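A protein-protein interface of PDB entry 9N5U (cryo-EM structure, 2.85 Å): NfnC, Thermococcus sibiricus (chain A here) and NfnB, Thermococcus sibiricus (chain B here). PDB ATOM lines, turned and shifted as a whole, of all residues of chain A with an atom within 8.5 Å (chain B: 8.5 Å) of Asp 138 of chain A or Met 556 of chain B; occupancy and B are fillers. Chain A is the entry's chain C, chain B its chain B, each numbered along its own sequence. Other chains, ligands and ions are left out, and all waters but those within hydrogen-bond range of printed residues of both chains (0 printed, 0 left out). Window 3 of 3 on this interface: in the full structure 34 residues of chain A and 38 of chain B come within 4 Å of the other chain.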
ATOM      1  N   ASN A  86     -23.621   7.414   0.814  1.00  0.00           N
ATOM      2  CA  ASN A  86     -23.251   7.204   2.211  1.00  0.00           C
ATOM      3  C   ASN A  86     -23.590   8.417   3.075  1.00  0.00           C
ATOM      4  O   ASN A  86     -24.086   8.264   4.199  1.00  0.00           O
ATOM      5  CB  ASN A  86     -21.765   6.869   2.315  1.00  0.00           C
ATOM      6  CG  ASN A  86     -21.416   5.557   1.641  1.00  0.00           C
ATOM      7  OD1 ASN A  86     -22.291   4.759   1.317  1.00  0.00           O
ATOM      8  ND2 ASN A  86     -20.127   5.325   1.436  1.00  0.00           N
ATOM      9  N   ILE A  87     -23.340   9.629   2.573  1.00  0.00           N
ATOM     10  CA  ILE A  87     -23.655  10.810   3.372  1.00  0.00           C
ATOM     11  C   ILE A  87     -25.165  11.019   3.469  1.00  0.00           C
ATOM     12  O   ILE A  87     -25.666  11.465   4.507  1.00  0.00           O
ATOM     13  CB  ILE A  87     -22.928  12.060   2.833  1.00  0.00           C
ATOM     14  CG1 ILE A  87     -23.512  12.530   1.503  1.00  0.00           C
ATOM     15  CG2 ILE A  87     -21.445  11.786   2.685  1.00  0.00           C
ATOM     16  CD1 ILE A  87     -22.900  13.810   0.994  1.00  0.00           C
ATOM     17  N   ALA A  90     -26.238   8.675   6.151  1.00  0.00           N
ATOM     18  CA  ALA A  90     -25.943   9.240   7.463  1.00  0.00           C
ATOM     19  C   ALA A  90     -26.959  10.309   7.852  1.00  0.00           C
ATOM     20  O   ALA A  90     -27.448  10.329   8.989  1.00  0.00           O
ATOM     21  CB  ALA A  90     -24.530   9.814   7.475  1.00  0.00           C
ATOM     22  N   GLU A  94     -29.577   9.894  10.975  1.00  0.00           N
ATOM     23  CA  GLU A  94     -29.538  10.811  12.113  1.00  0.00           C
ATOM     24  C   GLU A  94     -30.831  11.606  12.241  1.00  0.00           C
ATOM     25  O   GLU A  94     -31.336  11.806  13.350  1.00  0.00           O
ATOM     26  CB  GLU A  94     -28.346  11.759  11.991  1.00  0.00           C
ATOM     27  CG  GLU A  94     -27.004  11.097  12.202  1.00  0.00           C
ATOM     28  CD  GLU A  94     -26.825  10.577  13.614  1.00  0.00           C
ATOM     29  OE1 GLU A  94     -27.413  11.164  14.547  1.00  0.00           O
ATOM     30  OE2 GLU A  94     -26.095   9.579  13.792  1.00  0.00           O
ATOM     31  N   LYS A 134     -16.361  18.184   1.814  1.00  0.00           N
ATOM     32  CA  LYS A 134     -15.461  17.073   2.130  1.00  0.00           C
ATOM     33  C   LYS A 134     -16.041  16.206   3.249  1.00  0.00           C
ATOM     34  O   LYS A 134     -15.470  16.068   4.332  1.00  0.00           O
ATOM     35  CB  LYS A 134     -14.062  17.586   2.482  1.00  0.00           C
ATOM     36  CG  LYS A 134     -13.417  18.381   1.365  1.00  0.00           C
ATOM     37  CD  LYS A 134     -12.095  18.979   1.792  1.00  0.00           C
ATOM     38  CE  LYS A 134     -11.510  19.835   0.687  1.00  0.00           C
ATOM     39  NZ  LYS A 134     -11.335  19.060  -0.571  1.00  0.00           N
ATOM     40  N   LEU A 135     -17.191  15.612   2.957  1.00  0.00           N
ATOM     41  CA  LEU A 135     -18.014  14.951   3.965  1.00  0.00           C
ATOM     42  C   LEU A 135     -17.847  13.440   3.867  1.00  0.00           C
ATOM     43  O   LEU A 135     -18.377  12.801   2.958  1.00  0.00           O
ATOM     44  CB  LEU A 135     -19.476  15.344   3.797  1.00  0.00           C
ATOM     45  CG  LEU A 135     -19.829  16.817   3.959  1.00  0.00           C
ATOM     46  CD1 LEU A 135     -21.272  17.029   3.591  1.00  0.00           C
ATOM     47  CD2 LEU A 135     -19.568  17.277   5.379  1.00  0.00           C
ATOM     48  N   THR A 136     -17.108  12.876   4.805  1.00  0.00           N
ATOM     49  CA  THR A 136     -17.237  11.468   5.116  1.00  0.00           C
ATOM     50  C   THR A 136     -18.516  11.281   5.932  1.00  0.00           C
ATOM     51  O   THR A 136     -19.051  12.250   6.477  1.00  0.00           O
ATOM     52  CB  THR A 136     -15.999  10.994   5.876  1.00  0.00           C
ATOM     53  OG1 THR A 136     -15.864   9.574   5.764  1.00  0.00           O
ATOM     54  CG2 THR A 136     -16.086  11.368   7.344  1.00  0.00           C
ATOM     55  N   PRO A 137     -19.068  10.063   5.987  1.00  0.00           N
ATOM     56  CA  PRO A 137     -20.291   9.858   6.786  1.00  0.00           C
ATOM     57  C   PRO A 137     -20.166  10.267   8.245  1.00  0.00           C
ATOM     58  O   PRO A 137     -21.123  10.817   8.811  1.00  0.00           O
ATOM     59  CB  PRO A 137     -20.539   8.353   6.646  1.00  0.00           C
ATOM     60  CG  PRO A 137     -20.006   8.028   5.316  1.00  0.00           C
ATOM     61  CD  PRO A 137     -18.812   8.919   5.095  1.00  0.00           C
ATOM     62  N   ASP A 138     -19.010  10.031   8.869  1.00  0.00           N
ATOM     63  CA  ASP A 138     -18.817  10.433  10.260  1.00  0.00           C
ATOM     64  C   ASP A 138     -18.903  11.946  10.416  1.00  0.00           C
ATOM     65  O   ASP A 138     -19.530  12.450  11.358  1.00  0.00           O
ATOM     66  CB  ASP A 138     -17.469   9.910  10.758  1.00  0.00           C
ATOM     67  CG  ASP A 138     -17.232  10.191  12.228  1.00  0.00           C
ATOM     68  OD1 ASP A 138     -16.984  11.360  12.592  1.00  0.00           O
ATOM     69  OD2 ASP A 138     -17.295   9.235  13.027  1.00  0.00           O
ATOM     70  N   LYS A 139     -18.280  12.685   9.497  1.00  0.00           N
ATOM     71  CA  LYS A 139     -18.266  14.139   9.591  1.00  0.00           C
ATOM     72  C   LYS A 139     -19.666  14.716   9.433  1.00  0.00           C
ATOM     73  O   LYS A 139     -20.045  15.650  10.148  1.00  0.00           O
ATOM     74  CB  LYS A 139     -17.321  14.710   8.538  1.00  0.00           C
ATOM     75  CG  LYS A 139     -16.379  15.768   9.062  1.00  0.00           C
ATOM     76  CD  LYS A 139     -15.058  15.725   8.322  1.00  0.00           C
ATOM     77  CE  LYS A 139     -14.380  14.382   8.516  1.00  0.00           C
ATOM     78  NZ  LYS A 139     -13.045  14.338   7.866  1.00  0.00           N
ATOM     79  N   VAL A 140     -20.456  14.165   8.511  1.00  0.00           N
ATOM     80  CA  VAL A 140     -21.799  14.694   8.320  1.00  0.00           C
ATOM     81  C   VAL A 140     -22.708  14.292   9.477  1.00  0.00           C
ATOM     82  O   VAL A 140     -23.624  15.042   9.837  1.00  0.00           O
ATOM     83  CB  VAL A 140     -22.357  14.273   6.945  1.00  0.00           C
ATOM     84  CG1 VAL A 140     -22.611  12.793   6.878  1.00  0.00           C
ATOM     85  CG2 VAL A 140     -23.614  15.050   6.620  1.00  0.00           C
ATOM     86  N   ARG A 141     -22.468  13.133  10.102  1.00  0.00           N
ATOM     87  CA  ARG A 141     -23.207  12.810  11.322  1.00  0.00           C
ATOM     88  C   ARG A 141     -22.888  13.801  12.434  1.00  0.00           C
ATOM     89  O   ARG A 141     -23.785  14.242  13.165  1.00  0.00           O
ATOM     90  CB  ARG A 141     -22.899  11.384  11.774  1.00  0.00           C
ATOM     91  CG  ARG A 141     -23.631  10.330  10.978  1.00  0.00           C
ATOM     92  CD  ARG A 141     -23.379   8.938  11.513  1.00  0.00           C
ATOM     93  NE  ARG A 141     -24.009   7.931  10.670  1.00  0.00           N
ATOM     94  CZ  ARG A 141     -25.253   7.498  10.822  1.00  0.00           C
ATOM     95  NH1 ARG A 141     -26.027   7.945  11.796  1.00  0.00           N
ATOM     96  NH2 ARG A 141     -25.729   6.585   9.981  1.00  0.00           N
ATOM     97  N   LYS A 142     -21.612  14.169  12.566  1.00  0.00           N
ATOM     98  CA  LYS A 142     -21.231  15.190  13.536  1.00  0.00           C
ATOM     99  C   LYS A 142     -21.913  16.520  13.241  1.00  0.00           C
ATOM    100  O   LYS A 142     -22.395  17.197  14.156  1.00  0.00           O
ATOM    101  CB  LYS A 142     -19.713  15.354  13.540  1.00  0.00           C
ATOM    102  CG  LYS A 142     -19.225  16.633  14.177  1.00  0.00           C
ATOM    103  CD  LYS A 142     -17.717  16.739  14.081  1.00  0.00           C
ATOM    104  CE  LYS A 142     -17.045  15.560  14.759  1.00  0.00           C
ATOM    105  NZ  LYS A 142     -15.562  15.656  14.691  1.00  0.00           N
ATOM    106  N   ILE A 143     -21.966  16.907  11.966  1.00  0.00           N
ATOM    107  CA  ILE A 143     -22.576  18.182  11.597  1.00  0.00           C
ATOM    108  C   ILE A 143     -24.074  18.176  11.892  1.00  0.00           C
ATOM    109  O   ILE A 143     -24.622  19.160  12.399  1.00  0.00           O
ATOM    110  CB  ILE A 143     -22.275  18.506  10.122  1.00  0.00           C
ATOM    111  CG1 ILE A 143     -20.786  18.800   9.944  1.00  0.00           C
ATOM    112  CG2 ILE A 143     -23.094  19.688   9.646  1.00  0.00           C
ATOM    113  CD1 ILE A 143     -20.398  19.182   8.543  1.00  0.00           C
ATOM    114  N   ILE A 144     -24.758  17.067  11.600  1.00  0.00           N
ATOM    115  CA  ILE A 144     -26.187  16.981  11.897  1.00  0.00           C
ATOM    116  C   ILE A 144     -26.434  17.039  13.401  1.00  0.00           C
ATOM    117  O   ILE A 144     -27.338  17.744  13.870  1.00  0.00           O
ATOM    118  CB  ILE A 144     -26.791  15.709  11.274  1.00  0.00           C
ATOM    119  CG1 ILE A 144     -26.715  15.777   9.752  1.00  0.00           C
ATOM    120  CG2 ILE A 144     -28.230  15.532  11.706  1.00  0.00           C
ATOM    121  CD1 ILE A 144     -27.286  17.039   9.182  1.00  0.00           C
ATOM    122  N   ARG A 145     -25.638  16.302  14.182  1.00  0.00           N
ATOM    123  CA  ARG A 145     -25.853  16.285  15.625  1.00  0.00           C
ATOM    124  C   ARG A 145     -25.549  17.640  16.250  1.00  0.00           C
ATOM    125  O   ARG A 145     -26.224  18.055  17.198  1.00  0.00           O
ATOM    126  CB  ARG A 145     -25.017  15.185  16.274  1.00  0.00           C
ATOM    127  CG  ARG A 145     -25.590  13.795  16.072  1.00  0.00           C
ATOM    128  CD  ARG A 145     -25.162  12.857  17.179  1.00  0.00           C
ATOM    129  NE  ARG A 145     -23.747  12.526  17.104  1.00  0.00           N
ATOM    130  CZ  ARG A 145     -23.273  11.381  16.635  1.00  0.00           C
ATOM    131  NH1 ARG A 145     -24.078  10.427  16.199  1.00  0.00           N
ATOM    132  NH2 ARG A 145     -21.957  11.187  16.605  1.00  0.00           N
ATOM    133  N   THR B 551      -9.227  -0.361  18.667  1.00  0.00           N
ATOM    134  CA  THR B 551     -10.615  -0.295  18.206  1.00  0.00           C
ATOM    135  C   THR B 551     -11.000   1.129  17.798  1.00  0.00           C
ATOM    136  O   THR B 551     -11.916   1.742  18.351  1.00  0.00           O
ATOM    137  CB  THR B 551     -11.582  -0.850  19.261  1.00  0.00           C
ATOM    138  OG1 THR B 551     -11.634   0.034  20.388  1.00  0.00           O
ATOM    139  CG2 THR B 551     -11.137  -2.231  19.721  1.00  0.00           C
ATOM    140  N   ALA B 552     -10.266   1.650  16.813  1.00  0.00           N
ATOM    141  CA  ALA B 552     -10.588   2.967  16.273  1.00  0.00           C
ATOM    142  C   ALA B 552     -11.941   2.953  15.574  1.00  0.00           C
ATOM    143  O   ALA B 552     -12.725   3.901  15.694  1.00  0.00           O
ATOM    144  CB  ALA B 552      -9.486   3.432  15.320  1.00  0.00           C
ATOM    145  N   CYS B 553     -12.236   1.883  14.840  1.00  0.00           N
ATOM    146  CA  CYS B 553     -13.522   1.759  14.153  1.00  0.00           C
ATOM    147  C   CYS B 553     -14.556   1.047  15.021  1.00  0.00           C
ATOM    148  O   CYS B 553     -15.239   0.119  14.589  1.00  0.00           O
ATOM    149  CB  CYS B 553     -13.333   1.040  12.821  1.00  0.00           C
ATOM    150  SG  CYS B 553     -12.785  -0.681  12.954  1.00  0.00           S
ATOM    151  N   ALA B 554     -14.699   1.505  16.261  1.00  0.00           N
ATOM    152  CA  ALA B 554     -15.694   0.956  17.171  1.00  0.00           C
ATOM    153  C   ALA B 554     -16.567   2.007  17.834  1.00  0.00           C
ATOM    154  O   ALA B 554     -17.709   1.691  18.190  1.00  0.00           O
ATOM    155  CB  ALA B 554     -15.020   0.115  18.265  1.00  0.00           C
ATOM    156  N   ILE B 555     -16.079   3.237  18.011  1.00  0.00           N
ATOM    157  CA  ILE B 555     -16.902   4.313  18.554  1.00  0.00           C
ATOM    158  C   ILE B 555     -17.577   5.121  17.455  1.00  0.00           C
ATOM    159  O   ILE B 555     -18.587   5.792  17.719  1.00  0.00           O
ATOM    160  CB  ILE B 555     -16.054   5.240  19.450  1.00  0.00           C
ATOM    161  CG1 ILE B 555     -15.013   4.430  20.225  1.00  0.00           C
ATOM    162  CG2 ILE B 555     -16.935   6.007  20.423  1.00  0.00           C
ATOM    163  CD1 ILE B 555     -15.602   3.504  21.274  1.00  0.00           C
ATOM    164  N   MET B 556     -17.061   5.069  16.227  1.00  0.00           N
ATOM    165  CA  MET B 556     -17.626   5.826  15.119  1.00  0.00           C
ATOM    166  C   MET B 556     -18.811   5.131  14.463  1.00  0.00           C
ATOM    167  O   MET B 556     -19.642   5.803  13.842  1.00  0.00           O
ATOM    168  CB  MET B 556     -16.548   6.100  14.067  1.00  0.00           C
ATOM    169  CG  MET B 556     -15.452   7.035  14.545  1.00  0.00           C
ATOM    170  SD  MET B 556     -14.671   6.466  16.065  1.00  0.00           S
ATOM    171  CE  MET B 556     -14.746   7.954  17.056  1.00  0.00           C
ATOM    172  N   CYS B 557     -18.912   3.813  14.580  1.00  0.00           N
ATOM    173  CA  CYS B 557     -20.037   3.107  13.986  1.00  0.00           C
ATOM    174  C   CYS B 557     -21.318   3.444  14.744  1.00  0.00           C
ATOM    175  O   CYS B 557     -21.377   3.257  15.968  1.00  0.00           O
ATOM    176  CB  CYS B 557     -19.806   1.599  14.000  1.00  0.00           C
ATOM    177  SG  CYS B 557     -21.243   0.645  13.465  1.00  0.00           S
ATOM    178  N   PRO B 558     -22.356   3.936  14.066  1.00  0.00           N
ATOM    179  CA  PRO B 558     -23.598   4.299  14.755  1.00  0.00           C
ATOM    180  C   PRO B 558     -24.612   3.175  14.876  1.00  0.00           C
ATOM    181  O   PRO B 558     -25.574   3.320  15.641  1.00  0.00           O
ATOM    182  CB  PRO B 558     -24.148   5.417  13.863  1.00  0.00           C
ATOM    183  CG  PRO B 558     -23.725   4.993  12.493  1.00  0.00           C
ATOM    184  CD  PRO B 558     -22.378   4.330  12.647  1.00  0.00           C
ATOM    185  N   VAL B 559     -24.432   2.071  14.147  1.00  0.00           N
ATOM    186  CA  VAL B 559     -25.395   0.974  14.170  1.00  0.00           C
ATOM    187  C   VAL B 559     -25.024  -0.111  15.173  1.00  0.00           C
ATOM    188  O   VAL B 559     -25.837  -1.021  15.410  1.00  0.00           O
ATOM    189  CB  VAL B 559     -25.563   0.364  12.760  1.00  0.00           C
ATOM    190  CG1 VAL B 559     -24.500  -0.689  12.502  1.00  0.00           C
ATOM    191  CG2 VAL B 559     -26.967  -0.202  12.572  1.00  0.00           C
ATOM    192  N   LYS B 560     -23.837  -0.035  15.781  1.00  0.00           N
ATOM    193  CA  LYS B 560     -23.358  -1.010  16.764  1.00  0.00           C
ATOM    194  C   LYS B 560     -23.320  -2.419  16.168  1.00  0.00           C
ATOM    195  O   LYS B 560     -24.039  -3.329  16.587  1.00  0.00           O
ATOM    196  CB  LYS B 560     -24.205  -0.967  18.043  1.00  0.00           C
ATOM    197  CG  LYS B 560     -23.561  -1.651  19.243  1.00  0.00           C
ATOM    198  CD  LYS B 560     -24.559  -1.837  20.374  1.00  0.00           C
ATOM    199  CE  LYS B 560     -25.704  -2.745  19.954  1.00  0.00           C
ATOM    200  NZ  LYS B 560     -25.221  -4.092  19.537  1.00  0.00           N
ATOM    201  N   ILE B 562     -20.038  -3.653  15.559  1.00  0.00           N
ATOM    202  CA  ILE B 562     -18.623  -3.937  15.745  1.00  0.00           C
ATOM    203  C   ILE B 562     -18.398  -4.669  17.062  1.00  0.00           C
ATOM    204  O   ILE B 562     -19.241  -4.625  17.958  1.00  0.00           O
ATOM    205  CB  ILE B 562     -17.788  -2.648  15.689  1.00  0.00           C
ATOM    206  CG1 ILE B 562     -16.307  -2.960  15.907  1.00  0.00           C
ATOM    207  CG2 ILE B 562     -18.289  -1.650  16.721  1.00  0.00           C
ATOM    208  CD1 ILE B 562     -15.707  -3.851  14.843  1.00  0.00           C
ATOM    209  N   CYS B 580     -22.573   1.451   5.908  1.00  0.00           N
ATOM    210  CA  CYS B 580     -22.199   2.823   5.583  1.00  0.00           C
ATOM    211  C   CYS B 580     -20.779   2.895   5.039  1.00  0.00           C
ATOM    212  O   CYS B 580     -20.517   3.603   4.060  1.00  0.00           O
ATOM    213  CB  CYS B 580     -22.335   3.713   6.816  1.00  0.00           C
ATOM    214  SG  CYS B 580     -21.146   3.343   8.118  1.00  0.00           S
ATOM    215  N   GLY B 581     -19.853   2.171   5.653  1.00  0.00           N
ATOM    216  CA  GLY B 581     -18.471   2.182   5.233  1.00  0.00           C
ATOM    217  C   GLY B 581     -17.553   3.075   6.030  1.00  0.00           C
ATOM    218  O   GLY B 581     -16.402   3.265   5.623  1.00  0.00           O
ATOM    219  N   THR B 582     -18.017   3.632   7.150  1.00  0.00           N
ATOM    220  CA  THR B 582     -17.169   4.498   7.959  1.00  0.00           C
ATOM    221  C   THR B 582     -16.035   3.735   8.634  1.00  0.00           C
ATOM    222  O   THR B 582     -15.064   4.357   9.073  1.00  0.00           O
ATOM    223  CB  THR B 582     -18.008   5.217   9.012  1.00  0.00           C
ATOM    224  OG1 THR B 582     -19.323   5.449   8.492  1.00  0.00           O
ATOM    225  CG2 THR B 582     -17.380   6.550   9.363  1.00  0.00           C
ATOM    226  N   CYS B 583     -16.142   2.407   8.732  1.00  0.00           N
ATOM    227  CA  CYS B 583     -15.063   1.614   9.313  1.00  0.00           C
ATOM    228  C   CYS B 583     -13.790   1.713   8.485  1.00  0.00           C
ATOM    229  O   CYS B 583     -12.691   1.839   9.035  1.00  0.00           O
ATOM    230  CB  CYS B 583     -15.491   0.153   9.436  1.00  0.00           C
ATOM    231  SG  CYS B 583     -16.647  -0.181  10.765  1.00  0.00           S
ATOM    232  N   GLU B 585     -12.491   3.980   6.732  1.00  0.00           N
ATOM    233  CA  GLU B 585     -11.778   5.252   6.749  1.00  0.00           C
ATOM    234  C   GLU B 585     -11.229   5.616   8.120  1.00  0.00           C
ATOM    235  O   GLU B 585     -10.076   6.045   8.223  1.00  0.00           O
ATOM    236  CB  GLU B 585     -12.693   6.376   6.253  1.00  0.00           C
ATOM    237  CG  GLU B 585     -12.028   7.741   6.214  1.00  0.00           C
ATOM    238  CD  GLU B 585     -12.934   8.813   5.646  1.00  0.00           C
ATOM    239  OE1 GLU B 585     -13.995   8.459   5.090  1.00  0.00           O
ATOM    240  OE2 GLU B 585     -12.591  10.008   5.756  1.00  0.00           O
ATOM    241  N   VAL B 586     -12.024   5.452   9.184  1.00  0.00           N
ATOM    242  CA  VAL B 586     -11.593   5.852  10.521  1.00  0.00           C
ATOM    243  C   VAL B 586     -10.724   4.802  11.198  1.00  0.00           C
ATOM    244  O   VAL B 586     -10.245   5.037  12.315  1.00  0.00           O
ATOM    245  CB  VAL B 586     -12.800   6.171  11.425  1.00  0.00           C
ATOM    246  CG1 VAL B 586     -13.753   7.127  10.722  1.00  0.00           C
ATOM    247  CG2 VAL B 586     -13.513   4.892  11.838  1.00  0.00           C
ATOM    248  N   CYS B 587     -10.507   3.650  10.559  1.00  0.00           N
ATOM    249  CA  CYS B 587      -9.661   2.619  11.151  1.00  0.00           C
ATOM    250  C   CYS B 587      -8.206   3.051  11.253  1.00  0.00           C
ATOM    251  O   CYS B 587      -7.496   2.558  12.138  1.00  0.00           O
ATOM    252  CB  CYS B 587      -9.760   1.325  10.338  1.00  0.00           C
ATOM    253  SG  CYS B 587      -8.742  -0.050  10.945  1.00  0.00           S
ATOM    254  N   ARG B 588      -7.760   3.958  10.374  1.00  0.00           N
ATOM    255  CA  ARG B 588      -6.377   4.420  10.233  1.00  0.00           C
ATOM    256  C   ARG B 588      -5.380   3.269  10.352  1.00  0.00           C
ATOM    257  O   ARG B 588      -4.300   3.421  10.931  1.00  0.00           O
ATOM    258  CB  ARG B 588      -6.058   5.551  11.231  1.00  0.00           C
ATOM    259  CG  ARG B 588      -6.182   5.243  12.720  1.00  0.00           C
ATOM    260  CD  ARG B 588      -6.294   6.520  13.539  1.00  0.00           C
ATOM    261  NE  ARG B 588      -6.638   6.247  14.929  1.00  0.00           N
ATOM    262  CZ  ARG B 588      -6.925   7.180  15.826  1.00  0.00           C
ATOM    263  NH1 ARG B 588      -6.921   8.466  15.513  1.00  0.00           N
ATOM    264  NH2 ARG B 588      -7.227   6.816  17.069  1.00  0.00           N
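Along chain A the printed residues that touch a printed residue of chain B span positions 86 to 141.
Of the 19 printed residues of chain B, 5 touch a printed residue of chain A.
Printed residues of chain B that touch a printed residue of chain A: Met 556, Pro 558, Cys 580, Thr 582 and Glu 585.
Hydrophobic or aromatic side chains of chain B that line the printed part of chain A: Met 556 and Pro 558.
Among the printed residues, 6 pairs touch across the chains.
Among the printed residues, no Asp or Glu carboxylate lies within 4 Å of a Lys or Arg side-chain nitrogen of the other chain.
SG of Cys 580 of chain B lies close to OG1 of Thr 582 of chain B (2.8 Å).
The side-chain carboxylate (OE2) of Glu 94 of chain A is in salt-bridge range of the guanidinium group (NH1) of Arg 141 of chain A, at 2.6 Å.
Among the printed residues, merely in contact across the chains: Asp 138 of chain A with Met 556 of chain B (3.2 Å), Arg 141 of chain A with Pro 558 of chain B (3.4 Å), Asp 138 of chain A with Thr 582 of chain B (3.6 Å) and Pro 137 of chain A with Thr 582 of chain B (3.6 Å).
Of the printed residues of chain B, Asn 86 of chain A touches Cys 580 (3.2 Å).
Of the printed residues of chain B, Thr 136 of chain A touches Glu 585.
Asp 138 of chain A touches just these residues of chain B: Met 556 (3.2 Å) and Thr 582 (3.6 Å).
Of chain A, only Asp 138 comes within 4 Å of Met 556 of chain B.
Of the printed residues of chain A, Pro 558 of chain B touches Arg 141.
The nearest residue of chain A that does not touch Met 556 of chain B is Arg 141 of chain A (5.4 Å).
The side-chain amide nitrogen (ND2) of Asn 86 of chain A is in hydrogen-bond range of the backbone carbonyl oxygen (O) of Cys 580 of chain B, 3.2 Å away.
OE2 of Glu 585 of chain B lies close to OG1 of Thr 136 of chain A (3.3 Å).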
